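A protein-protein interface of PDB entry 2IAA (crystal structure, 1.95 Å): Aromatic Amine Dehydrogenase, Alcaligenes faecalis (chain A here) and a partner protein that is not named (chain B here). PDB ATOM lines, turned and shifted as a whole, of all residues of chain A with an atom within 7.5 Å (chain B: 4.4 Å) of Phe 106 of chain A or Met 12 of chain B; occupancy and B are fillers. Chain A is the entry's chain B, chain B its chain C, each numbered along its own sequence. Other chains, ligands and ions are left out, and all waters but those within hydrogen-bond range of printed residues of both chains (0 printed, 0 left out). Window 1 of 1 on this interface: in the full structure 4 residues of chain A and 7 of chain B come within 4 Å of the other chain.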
ATOM      1  N   PRO A  59      -6.380 -23.498 -12.055  1.00  0.00           N
ATOM      2  CA  PRO A  59      -4.966 -23.567 -12.439  1.00  0.00           C
ATOM      3  C   PRO A  59      -4.817 -23.637 -13.956  1.00  0.00           C
ATOM      4  O   PRO A  59      -3.797 -23.238 -14.516  1.00  0.00           O
ATOM      5  CB  PRO A  59      -4.489 -24.840 -11.754  1.00  0.00           C
ATOM      6  CG  PRO A  59      -5.713 -25.719 -11.831  1.00  0.00           C
ATOM      7  CD  PRO A  59      -6.823 -24.760 -11.435  1.00  0.00           C
ATOM      8  N   ILE A  60      -5.853 -24.141 -14.615  1.00  0.00           N
ATOM      9  CA  ILE A  60      -5.847 -24.286 -16.062  1.00  0.00           C
ATOM     10  C   ILE A  60      -6.759 -23.262 -16.722  1.00  0.00           C
ATOM     11  O   ILE A  60      -7.512 -22.553 -16.046  1.00  0.00           O
ATOM     12  CB  ILE A  60      -6.294 -25.705 -16.465  1.00  0.00           C
ATOM     13  CG1 ILE A  60      -7.636 -26.029 -15.803  1.00  0.00           C
ATOM     14  CG2 ILE A  60      -5.232 -26.718 -16.040  1.00  0.00           C
ATOM     15  CD1 ILE A  60      -8.168 -27.401 -16.119  1.00  0.00           C
ATOM     16  N   SER A  61      -6.693 -23.187 -18.047  1.00  0.00           N
ATOM     17  CA  SER A  61      -7.509 -22.228 -18.772  1.00  0.00           C
ATOM     18  C   SER A  61      -7.394 -22.396 -20.271  1.00  0.00           C
ATOM     19  O   SER A  61      -6.595 -23.195 -20.774  1.00  0.00           O
ATOM     20  CB  SER A  61      -7.061 -20.812 -18.420  1.00  0.00           C
ATOM     21  OG  SER A  61      -5.744 -20.582 -18.902  1.00  0.00           O
ATOM     22  N   TRQ A  62      -8.217 -21.646 -20.989  1.00  0.00           N
ATOM     23  CA  TRQ A  62      -8.142 -21.665 -22.429  1.00  0.00           C
ATOM     24  C   TRQ A  62      -7.369 -20.383 -22.753  1.00  0.00           C
ATOM     25  O   TRQ A  62      -7.378 -19.430 -21.971  1.00  0.00           O
ATOM     26  CB  TRQ A  62      -9.549 -21.721 -23.061  1.00  0.00           C
ATOM     27  CG  TRQ A  62     -10.520 -20.619 -22.715  1.00  0.00           C
ATOM     28  CD1 TRQ A  62     -10.619 -19.414 -23.355  1.00  0.00           C
ATOM     29  NE1 TRQ A  62     -11.655 -18.684 -22.838  1.00  0.00           N
ATOM     30  CE2 TRQ A  62     -12.254 -19.402 -21.841  1.00  0.00           C
ATOM     31  CZ2 TRQ A  62     -13.344 -19.051 -21.038  1.00  0.00           C
ATOM     32  CH2 TRQ A  62     -13.756 -19.953 -20.092  1.00  0.00           C
ATOM     33  CZ3 TRQ A  62     -13.117 -21.194 -19.932  1.00  0.00           C
ATOM     34  CE3 TRQ A  62     -12.033 -21.555 -20.731  1.00  0.00           C
ATOM     35  CD2 TRQ A  62     -11.575 -20.646 -21.719  1.00  0.00           C
ATOM     36  O6  TRQ A  62     -14.696 -19.581 -19.374  1.00  0.00           O
ATOM     37  O7  TRQ A  62     -13.938 -17.973 -21.184  1.00  0.00           O
ATOM     38  N   ILE A  63      -6.666 -20.364 -23.875  1.00  0.00           N
ATOM     39  CA  ILE A  63      -5.878 -19.191 -24.222  1.00  0.00           C
ATOM     40  C   ILE A  63      -6.309 -18.537 -25.525  1.00  0.00           C
ATOM     41  O   ILE A  63      -6.793 -19.203 -26.439  1.00  0.00           O
ATOM     42  CB  ILE A  63      -4.384 -19.562 -24.303  1.00  0.00           C
ATOM     43  CG1 ILE A  63      -3.923 -20.092 -22.944  1.00  0.00           C
ATOM     44  CG2 ILE A  63      -3.556 -18.351 -24.693  1.00  0.00           C
ATOM     45  CD1 ILE A  63      -2.523 -20.637 -22.944  1.00  0.00           C
ATOM     46  N   GLY A  64      -6.137 -17.224 -25.593  1.00  0.00           N
ATOM     47  CA  GLY A  64      -6.506 -16.496 -26.789  1.00  0.00           C
ATOM     48  C   GLY A  64      -5.460 -15.478 -27.204  1.00  0.00           C
ATOM     49  O   GLY A  64      -4.684 -14.990 -26.383  1.00  0.00           O
ATOM     50  N   ILE A  77      -3.519 -13.926 -24.153  1.00  0.00           N
ATOM     51  CA  ILE A  77      -4.339 -13.765 -22.954  1.00  0.00           C
ATOM     52  C   ILE A  77      -4.715 -15.139 -22.419  1.00  0.00           C
ATOM     53  O   ILE A  77      -5.119 -16.017 -23.184  1.00  0.00           O
ATOM     54  CB  ILE A  77      -5.649 -12.997 -23.259  1.00  0.00           C
ATOM     55  CG1 ILE A  77      -5.338 -11.688 -23.996  1.00  0.00           C
ATOM     56  CG2 ILE A  77      -6.413 -12.732 -21.963  1.00  0.00           C
ATOM     57  CD1 ILE A  77      -4.463 -10.723 -23.227  1.00  0.00           C
ATOM     58  N   TYR A  79      -7.243 -17.196 -20.115  1.00  0.00           N
ATOM     59  CA  TYR A  79      -8.556 -17.088 -19.490  1.00  0.00           C
ATOM     60  C   TYR A  79      -8.836 -18.075 -18.366  1.00  0.00           C
ATOM     61  O   TYR A  79      -9.472 -19.110 -18.571  1.00  0.00           O
ATOM     62  CB  TYR A  79      -9.641 -17.196 -20.559  1.00  0.00           C
ATOM     63  CG  TYR A  79      -9.543 -16.094 -21.579  1.00  0.00           C
ATOM     64  CD1 TYR A  79      -8.924 -16.308 -22.812  1.00  0.00           C
ATOM     65  CD2 TYR A  79     -10.033 -14.820 -21.296  1.00  0.00           C
ATOM     66  CE1 TYR A  79      -8.799 -15.279 -23.736  1.00  0.00           C
ATOM     67  CE2 TYR A  79      -9.913 -13.786 -22.210  1.00  0.00           C
ATOM     68  CZ  TYR A  79      -9.297 -14.018 -23.426  1.00  0.00           C
ATOM     69  OH  TYR A  79      -9.195 -12.994 -24.329  1.00  0.00           O
ATOM     70  N   ARG A 100     -10.883 -22.126 -31.001  1.00  0.00           N
ATOM     71  CA  ARG A 100     -10.957 -23.321 -31.834  1.00  0.00           C
ATOM     72  C   ARG A 100     -11.670 -24.471 -31.115  1.00  0.00           C
ATOM     73  O   ARG A 100     -11.848 -24.434 -29.895  1.00  0.00           O
ATOM     74  CB  ARG A 100      -9.542 -23.732 -32.251  1.00  0.00           C
ATOM     75  CG  ARG A 100      -8.857 -22.709 -33.157  1.00  0.00           C
ATOM     76  CD  ARG A 100      -9.531 -22.652 -34.529  1.00  0.00           C
ATOM     77  NE  ARG A 100      -8.874 -21.733 -35.462  1.00  0.00           N
ATOM     78  CZ  ARG A 100      -9.093 -20.422 -35.522  1.00  0.00           C
ATOM     79  NH1 ARG A 100      -9.957 -19.846 -34.697  1.00  0.00           N
ATOM     80  NH2 ARG A 100      -8.462 -19.684 -36.430  1.00  0.00           N
ATOM     81  N   PRO A 101     -12.098 -25.503 -31.864  1.00  0.00           N
ATOM     82  CA  PRO A 101     -12.799 -26.660 -31.290  1.00  0.00           C
ATOM     83  C   PRO A 101     -12.010 -27.506 -30.285  1.00  0.00           C
ATOM     84  O   PRO A 101     -10.807 -27.316 -30.095  1.00  0.00           O
ATOM     85  CB  PRO A 101     -13.205 -27.469 -32.524  1.00  0.00           C
ATOM     86  CG  PRO A 101     -13.340 -26.417 -33.593  1.00  0.00           C
ATOM     87  CD  PRO A 101     -12.125 -25.559 -33.336  1.00  0.00           C
ATOM     88  N   GLY A 102     -12.712 -28.448 -29.657  1.00  0.00           N
ATOM     89  CA  GLY A 102     -12.120 -29.322 -28.658  1.00  0.00           C
ATOM     90  C   GLY A 102     -10.890 -30.117 -29.055  1.00  0.00           C
ATOM     91  O   GLY A 102     -10.138 -30.556 -28.181  1.00  0.00           O
ATOM     92  N   TYR A 103     -10.675 -30.326 -30.350  1.00  0.00           N
ATOM     93  CA  TYR A 103      -9.495 -31.066 -30.783  1.00  0.00           C
ATOM     94  C   TYR A 103      -8.228 -30.205 -30.677  1.00  0.00           C
ATOM     95  O   TYR A 103      -7.121 -30.663 -30.958  1.00  0.00           O
ATOM     96  CB  TYR A 103      -9.699 -31.634 -32.193  1.00  0.00           C
ATOM     97  CG  TYR A 103     -10.147 -30.650 -33.247  1.00  0.00           C
ATOM     98  CD1 TYR A 103      -9.244 -29.758 -33.828  1.00  0.00           C
ATOM     99  CD2 TYR A 103     -11.466 -30.643 -33.698  1.00  0.00           C
ATOM    100  CE1 TYR A 103      -9.643 -28.888 -34.836  1.00  0.00           C
ATOM    101  CE2 TYR A 103     -11.879 -29.774 -34.711  1.00  0.00           C
ATOM    102  CZ  TYR A 103     -10.957 -28.901 -35.274  1.00  0.00           C
ATOM    103  OH  TYR A 103     -11.346 -28.046 -36.281  1.00  0.00           O
ATOM    104  N   GLU A 104      -8.419 -28.953 -30.265  1.00  0.00           N
ATOM    105  CA  GLU A 104      -7.337 -27.990 -30.001  1.00  0.00           C
ATOM    106  C   GLU A 104      -7.816 -27.456 -28.657  1.00  0.00           C
ATOM    107  O   GLU A 104      -8.051 -26.256 -28.486  1.00  0.00           O
ATOM    108  CB  GLU A 104      -7.324 -26.842 -31.012  1.00  0.00           C
ATOM    109  CG  GLU A 104      -6.891 -27.215 -32.409  1.00  0.00           C
ATOM    110  CD  GLU A 104      -6.560 -25.993 -33.247  1.00  0.00           C
ATOM    111  OE1 GLU A 104      -5.533 -25.334 -32.962  1.00  0.00           O
ATOM    112  OE2 GLU A 104      -7.331 -25.688 -34.186  1.00  0.00           O
ATOM    113  N   PHE A 105      -7.969 -28.385 -27.720  1.00  0.00           N
ATOM    114  CA  PHE A 105      -8.514 -28.120 -26.398  1.00  0.00           C
ATOM    115  C   PHE A 105      -8.194 -26.840 -25.642  1.00  0.00           C
ATOM    116  O   PHE A 105      -9.110 -26.178 -25.159  1.00  0.00           O
ATOM    117  CB  PHE A 105      -8.253 -29.319 -25.483  1.00  0.00           C
ATOM    118  CG  PHE A 105      -9.329 -29.528 -24.454  1.00  0.00           C
ATOM    119  CD1 PHE A 105     -10.658 -29.688 -24.847  1.00  0.00           C
ATOM    120  CD2 PHE A 105      -9.026 -29.549 -23.098  1.00  0.00           C
ATOM    121  CE1 PHE A 105     -11.668 -29.866 -23.902  1.00  0.00           C
ATOM    122  CE2 PHE A 105     -10.031 -29.728 -22.146  1.00  0.00           C
ATOM    123  CZ  PHE A 105     -11.353 -29.886 -22.549  1.00  0.00           C
ATOM    124  N   PHE A 106      -6.924 -26.470 -25.532  1.00  0.00           N
ATOM    125  CA  PHE A 106      -6.607 -25.267 -24.776  1.00  0.00           C
ATOM    126  C   PHE A 106      -6.878 -23.948 -25.485  1.00  0.00           C
ATOM    127  O   PHE A 106      -6.569 -22.877 -24.961  1.00  0.00           O
ATOM    128  CB  PHE A 106      -5.174 -25.340 -24.249  1.00  0.00           C
ATOM    129  CG  PHE A 106      -4.954 -26.496 -23.314  1.00  0.00           C
ATOM    130  CD1 PHE A 106      -4.447 -27.703 -23.788  1.00  0.00           C
ATOM    131  CD2 PHE A 106      -5.349 -26.410 -21.980  1.00  0.00           C
ATOM    132  CE1 PHE A 106      -4.341 -28.813 -22.951  1.00  0.00           C
ATOM    133  CE2 PHE A 106      -5.248 -27.516 -21.134  1.00  0.00           C
ATOM    134  CZ  PHE A 106      -4.745 -28.720 -21.622  1.00  0.00           C
ATOM    135  N   LEU A 107      -7.476 -24.035 -26.667  1.00  0.00           N
ATOM    136  CA  LEU A 107      -7.852 -22.853 -27.431  1.00  0.00           C
ATOM    137  C   LEU A 107      -9.378 -22.858 -27.514  1.00  0.00           C
ATOM    138  O   LEU A 107      -9.978 -22.033 -28.201  1.00  0.00           O
ATOM    139  CB  LEU A 107      -7.279 -22.909 -28.851  1.00  0.00           C
ATOM    140  CG  LEU A 107      -5.759 -22.985 -29.042  1.00  0.00           C
ATOM    141  CD1 LEU A 107      -5.435 -22.960 -30.539  1.00  0.00           C
ATOM    142  CD2 LEU A 107      -5.084 -21.825 -28.339  1.00  0.00           C
ATOM    143  N   HIS A 108      -9.994 -23.796 -26.798  1.00  0.00           N
ATOM    144  CA  HIS A 108     -11.447 -23.977 -26.800  1.00  0.00           C
ATOM    145  C   HIS A 108     -12.142 -23.348 -25.590  1.00  0.00           C
ATOM    146  O   HIS A 108     -11.761 -23.611 -24.452  1.00  0.00           O
ATOM    147  CB  HIS A 108     -11.752 -25.478 -26.831  1.00  0.00           C
ATOM    148  CG  HIS A 108     -13.191 -25.803 -27.078  1.00  0.00           C
ATOM    149  ND1 HIS A 108     -13.825 -26.869 -26.475  1.00  0.00           N
ATOM    150  CD2 HIS A 108     -14.105 -25.237 -27.899  1.00  0.00           C
ATOM    151  CE1 HIS A 108     -15.066 -26.947 -26.916  1.00  0.00           C
ATOM    152  NE2 HIS A 108     -15.261 -25.969 -27.783  1.00  0.00           N
ATOM    153  N   ASN A 109     -13.172 -22.538 -25.823  1.00  0.00           N
ATOM    154  CA  ASN A 109     -13.867 -21.910 -24.701  1.00  0.00           C
ATOM    155  C   ASN A 109     -15.317 -22.359 -24.494  1.00  0.00           C
ATOM    156  O   ASN A 109     -16.092 -21.674 -23.826  1.00  0.00           O
ATOM    157  CB  ASN A 109     -13.790 -20.374 -24.797  1.00  0.00           C
ATOM    158  CG  ASN A 109     -14.682 -19.792 -25.889  1.00  0.00           C
ATOM    159  OD1 ASN A 109     -15.470 -20.500 -26.519  1.00  0.00           O
ATOM    160  ND2 ASN A 109     -14.563 -18.486 -26.108  1.00  0.00           N
ATOM    161  N   VAL A 111     -15.991 -25.116 -22.987  1.00  0.00           N
ATOM    162  CA  VAL A 111     -15.872 -26.034 -21.865  1.00  0.00           C
ATOM    163  C   VAL A 111     -15.597 -25.212 -20.603  1.00  0.00           C
ATOM    164  O   VAL A 111     -15.088 -24.090 -20.675  1.00  0.00           O
ATOM    165  CB  VAL A 111     -14.725 -27.053 -22.069  1.00  0.00           C
ATOM    166  CG1 VAL A 111     -15.060 -27.982 -23.229  1.00  0.00           C
ATOM    167  CG2 VAL A 111     -13.406 -26.321 -22.327  1.00  0.00           C
ATOM    168  N   TRP A 113     -13.571 -24.159 -17.722  1.00  0.00           N
ATOM    169  CA  TRP A 113     -12.183 -24.248 -17.299  1.00  0.00           C
ATOM    170  C   TRP A 113     -12.013 -24.386 -15.779  1.00  0.00           C
ATOM    171  O   TRP A 113     -10.918 -24.260 -15.244  1.00  0.00           O
ATOM    172  CB  TRP A 113     -11.356 -23.095 -17.906  1.00  0.00           C
ATOM    173  CG  TRP A 113     -10.963 -23.423 -19.352  1.00  0.00           C
ATOM    174  CD1 TRP A 113     -11.380 -22.788 -20.520  1.00  0.00           C
ATOM    175  CD2 TRP A 113     -10.213 -24.572 -19.777  1.00  0.00           C
ATOM    176  NE1 TRP A 113     -10.947 -23.500 -21.615  1.00  0.00           N
ATOM    177  CE2 TRP A 113     -10.228 -24.590 -21.192  1.00  0.00           C
ATOM    178  CE3 TRP A 113      -9.530 -25.591 -19.096  1.00  0.00           C
ATOM    179  CZ2 TRP A 113      -9.588 -25.588 -21.935  1.00  0.00           C
ATOM    180  CZ3 TRP A 113      -8.892 -26.585 -19.839  1.00  0.00           C
ATOM    181  CH2 TRP A 113      -8.928 -26.573 -21.242  1.00  0.00           C
ATOM    182  N   MET A 115     -13.261 -27.171 -14.557  1.00  0.00           N
ATOM    183  CA  MET A 115     -13.387 -28.629 -14.546  1.00  0.00           C
ATOM    184  C   MET A 115     -12.478 -29.443 -13.624  1.00  0.00           C
ATOM    185  O   MET A 115     -12.850 -30.547 -13.226  1.00  0.00           O
ATOM    186  CB  MET A 115     -13.253 -29.177 -15.970  1.00  0.00           C
ATOM    187  CG  MET A 115     -11.856 -29.039 -16.565  1.00  0.00           C
ATOM    188  SD  MET A 115     -11.726 -29.742 -18.221  1.00  0.00           S
ATOM    189  CE  MET A 115     -12.208 -28.339 -19.243  1.00  0.00           C
ATOM    190  N   ASN B   9       4.253 -26.916 -13.770  1.00  0.00           N
ATOM    191  CA  ASN B   9       3.158 -26.849 -12.803  1.00  0.00           C
ATOM    192  C   ASN B   9       1.789 -27.255 -13.349  1.00  0.00           C
ATOM    193  O   ASN B   9       1.669 -27.707 -14.488  1.00  0.00           O
ATOM    194  CB  ASN B   9       3.058 -25.434 -12.230  1.00  0.00           C
ATOM    195  CG  ASN B   9       2.906 -24.379 -13.310  1.00  0.00           C
ATOM    196  OD1 ASN B   9       2.265 -24.611 -14.337  1.00  0.00           O
ATOM    197  ND2 ASN B   9       3.485 -23.208 -13.078  1.00  0.00           N
ATOM    198  N   ASP B  10       0.763 -27.079 -12.515  1.00  0.00           N
ATOM    199  CA  ASP B  10      -0.613 -27.410 -12.881  1.00  0.00           C
ATOM    200  C   ASP B  10      -1.169 -26.403 -13.880  1.00  0.00           C
ATOM    201  O   ASP B  10      -2.279 -26.566 -14.388  1.00  0.00           O
ATOM    202  CB  ASP B  10      -1.518 -27.428 -11.642  1.00  0.00           C
ATOM    203  CG  ASP B  10      -1.214 -28.585 -10.703  1.00  0.00           C
ATOM    204  OD1 ASP B  10      -1.050 -29.724 -11.192  1.00  0.00           O
ATOM    205  OD2 ASP B  10      -1.154 -28.354  -9.475  1.00  0.00           O
ATOM    206  N   SER B  11      -0.397 -25.358 -14.152  1.00  0.00           N
ATOM    207  CA  SER B  11      -0.816 -24.321 -15.085  1.00  0.00           C
ATOM    208  C   SER B  11      -0.179 -24.487 -16.460  1.00  0.00           C
ATOM    209  O   SER B  11      -0.188 -23.559 -17.272  1.00  0.00           O
ATOM    210  CB  SER B  11      -0.484 -22.938 -14.523  1.00  0.00           C
ATOM    211  OG  SER B  11      -1.260 -22.665 -13.369  1.00  0.00           O
ATOM    212  N   MET B  12       0.385 -25.665 -16.710  1.00  0.00           N
ATOM    213  CA  MET B  12       1.003 -25.958 -17.998  1.00  0.00           C
ATOM    214  C   MET B  12       2.115 -24.971 -18.334  1.00  0.00           C
ATOM    215  O   MET B  12       2.152 -24.406 -19.429  1.00  0.00           O
ATOM    216  CB  MET B  12      -0.077 -25.922 -19.078  1.00  0.00           C
ATOM    217  CG  MET B  12       0.284 -26.604 -20.379  1.00  0.00           C
ATOM    218  SD  MET B  12      -1.229 -26.890 -21.322  1.00  0.00           S
ATOM    219  CE  MET B  12      -2.153 -27.831 -20.102  1.00  0.00           C
ATOM    220  N   GLN B  13       3.027 -24.765 -17.388  1.00  0.00           N
ATOM    221  CA  GLN B  13       4.123 -23.825 -17.599  1.00  0.00           C
ATOM    222  C   GLN B  13       5.460 -24.399 -17.171  1.00  0.00           C
ATOM    223  O   GLN B  13       5.549 -25.160 -16.205  1.00  0.00           O
ATOM    224  CB  GLN B  13       3.902 -22.548 -16.798  1.00  0.00           C
ATOM    225  CG  GLN B  13       2.554 -21.881 -16.981  1.00  0.00           C
ATOM    226  CD  GLN B  13       2.350 -20.722 -16.016  1.00  0.00           C
ATOM    227  OE1 GLN B  13       2.433 -20.889 -14.797  1.00  0.00           O
ATOM    228  NE2 GLN B  13       2.085 -19.541 -16.559  1.00  0.00           N
ATOM    229  N   MET B  43      -2.707 -34.087 -15.855  1.00  0.00           N
ATOM    230  CA  MET B  43      -1.812 -32.969 -16.137  1.00  0.00           C
ATOM    231  C   MET B  43      -0.340 -33.384 -16.053  1.00  0.00           C
ATOM    232  O   MET B  43       0.410 -32.882 -15.216  1.00  0.00           O
ATOM    233  CB  MET B  43      -2.106 -31.840 -15.141  1.00  0.00           C
ATOM    234  CG  MET B  43      -1.237 -30.600 -15.264  1.00  0.00           C
ATOM    235  SD  MET B  43      -1.344 -29.821 -16.869  1.00  0.00           S
ATOM    236  CE  MET B  43      -3.023 -29.175 -16.818  1.00  0.00           C
ATOM    237  N   HIS B  45       3.656 -33.928 -17.475  1.00  0.00           N
ATOM    238  CA  HIS B  45       4.645 -33.165 -18.231  1.00  0.00           C
ATOM    239  C   HIS B  45       5.868 -34.019 -18.547  1.00  0.00           C
ATOM    240  O   HIS B  45       6.170 -34.987 -17.844  1.00  0.00           O
ATOM    241  CB  HIS B  45       5.117 -31.942 -17.441  1.00  0.00           C
ATOM    242  CG  HIS B  45       4.022 -31.006 -17.041  1.00  0.00           C
ATOM    243  ND1 HIS B  45       3.142 -30.454 -17.947  1.00  0.00           N
ATOM    244  CD2 HIS B  45       3.693 -30.486 -15.835  1.00  0.00           C
ATOM    245  CE1 HIS B  45       2.320 -29.634 -17.317  1.00  0.00           C
ATOM    246  NE2 HIS B  45       2.633 -29.636 -16.035  1.00  0.00           N
ATOM    247  N   PRO B 114      -0.289 -34.451 -24.793  1.00  0.00           N
ATOM    248  CA  PRO B 114      -1.416 -33.935 -25.580  1.00  0.00           C
ATOM    249  C   PRO B 114      -1.859 -32.489 -25.330  1.00  0.00           C
ATOM    250  O   PRO B 114      -2.390 -32.154 -24.272  1.00  0.00           O
ATOM    251  CB  PRO B 114      -2.513 -34.951 -25.285  1.00  0.00           C
ATOM    252  CG  PRO B 114      -1.739 -36.231 -25.275  1.00  0.00           C
ATOM    253  CD  PRO B 114      -0.506 -35.869 -24.451  1.00  0.00           C
ATOM    254  N   GLY B 115      -1.622 -31.639 -26.327  1.00  0.00           N
ATOM    255  CA  GLY B 115      -2.008 -30.241 -26.244  1.00  0.00           C
ATOM    256  C   GLY B 115      -1.119 -29.318 -25.430  1.00  0.00           C
ATOM    257  O   GLY B 115      -1.375 -28.114 -25.380  1.00  0.00           O
ATOM    258  N   HIS B 116      -0.070 -29.851 -24.808  1.00  0.00           N
ATOM    259  CA  HIS B 116       0.812 -29.026 -23.987  1.00  0.00           C
ATOM    260  C   HIS B 116       1.941 -28.300 -24.710  1.00  0.00           C
ATOM    261  O   HIS B 116       2.370 -27.234 -24.265  1.00  0.00           O
ATOM    262  CB  HIS B 116       1.406 -29.853 -22.841  1.00  0.00           C
ATOM    263  CG  HIS B 116       0.396 -30.286 -21.823  1.00  0.00           C
ATOM    264  ND1 HIS B 116       0.746 -30.696 -20.554  1.00  0.00           N
ATOM    265  CD2 HIS B 116      -0.952 -30.382 -21.889  1.00  0.00           C
ATOM    266  CE1 HIS B 116      -0.342 -31.025 -19.883  1.00  0.00           C
ATOM    267  NE2 HIS B 116      -1.387 -30.844 -20.670  1.00  0.00           N
ATOM    268  N   ILE B 119       2.262 -24.093 -25.092  1.00  0.00           N
ATOM    269  CA  ILE B 119       2.999 -23.139 -24.271  1.00  0.00           C
ATOM    270  C   ILE B 119       4.299 -23.718 -23.736  1.00  0.00           C
ATOM    271  O   ILE B 119       5.314 -23.024 -23.666  1.00  0.00           O
ATOM    272  CB  ILE B 119       2.158 -22.656 -23.067  1.00  0.00           C
ATOM    273  CG1 ILE B 119       1.200 -21.553 -23.517  1.00  0.00           C
ATOM    274  CG2 ILE B 119       3.071 -22.156 -21.946  1.00  0.00           C
ATOM    275  CD1 ILE B 119       0.547 -20.814 -22.369  1.00  0.00           C
ATOM    276  N   MET B 120       4.264 -24.988 -23.352  1.00  0.00           N
ATOM    277  CA  MET B 120       5.442 -25.645 -22.811  1.00  0.00           C
ATOM    278  C   MET B 120       6.458 -26.001 -23.893  1.00  0.00           C
ATOM    279  O   MET B 120       6.582 -27.158 -24.299  1.00  0.00           O
ATOM    280  CB  MET B 120       5.022 -26.889 -22.029  1.00  0.00           C
ATOM    281  CG  MET B 120       4.059 -26.564 -20.897  1.00  0.00           C
ATOM    282  SD  MET B 120       3.656 -27.966 -19.858  1.00  0.00           S
ATOM    283  CE  MET B 120       4.974 -27.871 -18.656  1.00  0.00           C
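O of Pro 59 of chain A lies within hydrogen-bond range of OG of Ser 11 of chain B, at 2.8 Å.
Of the 21 printed residues of chain A, 4 touch a printed residue of chain B. Printed residues of chain A that touch a printed residue of chain B: Pro 59, Ile 60, Ile 63 and Phe 106. Printed residues of chain B that touch a printed residue of chain A: Asp 10, Ser 11, Met 12, Met 43, Gly 115, His 116 and Ile 119. Hydrophobic or aromatic side chains of chain B that line the printed part of chain A: Met 12, Met 43, His 116 and Ile 119. Among the printed residues, no Asp or Glu carboxylate lies within 4 Å of a Lys or Arg side-chain nitrogen of the other chain.
Of the printed residues of chain B, Ile 63 of chain A touches Ile 119. Tyr 103 of chain A touches none of the printed residues of chain B. Of chain B, only Met 12, Gly 115 and His 116 come within 4 Å of Phe 106 of chain A. Of the printed residues of chain A, Asp 10 of chain B touches Pro 59 (3.7 Å) and Ile 60 (3.4 Å). Printed residues of chain A within 4 Å of Ser 11 of chain B: Pro 59. Of the printed residues of chain A, Met 12 of chain B touches Phe 106. Of the printed residues of chain A, Ile 119 of chain B touches Ile 63 (3.1 Å). The nearest printed residue of chain B that does not touch Ile 63 of chain A is Met 12 of chain B (6.6 Å).
The backbone NH (N) of Ile 63 of chain A sits at hydrogen-bond distance from the backbone carbonyl oxygen (O) of Phe 106 of chain A (2.7 Å). The side-chain amide oxygen (OD1) of Asn 9 of chain B lies within hydrogen-bond range of the backbone NH (N) of Ser 11 of chain B. N of Met 12 of chain B sits at hydrogen-bond distance from OD1 of Asn 9 of chain B.
O of Pro 59 of chain A touches O of Asp 10 of chain B, 3.7 Å away. Ile 60 of chain A touches Asp 10 of chain B (CG2 to O, 3.4 Å). CE of Met 43 of chain B touches CG2 of Ile 60 of chain A, at 3.4 Å. Ile 63 of chain A touches Ile 119 of chain B. Met 12 of chain B touches Phe 106 of chain A. Phe 106 of chain A touches Gly 115 of chain B (CD1 to O, 3.5 Å). His 116 of chain B touches Phe 106 of chain A (CD2 to CE1, 3.9 Å).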
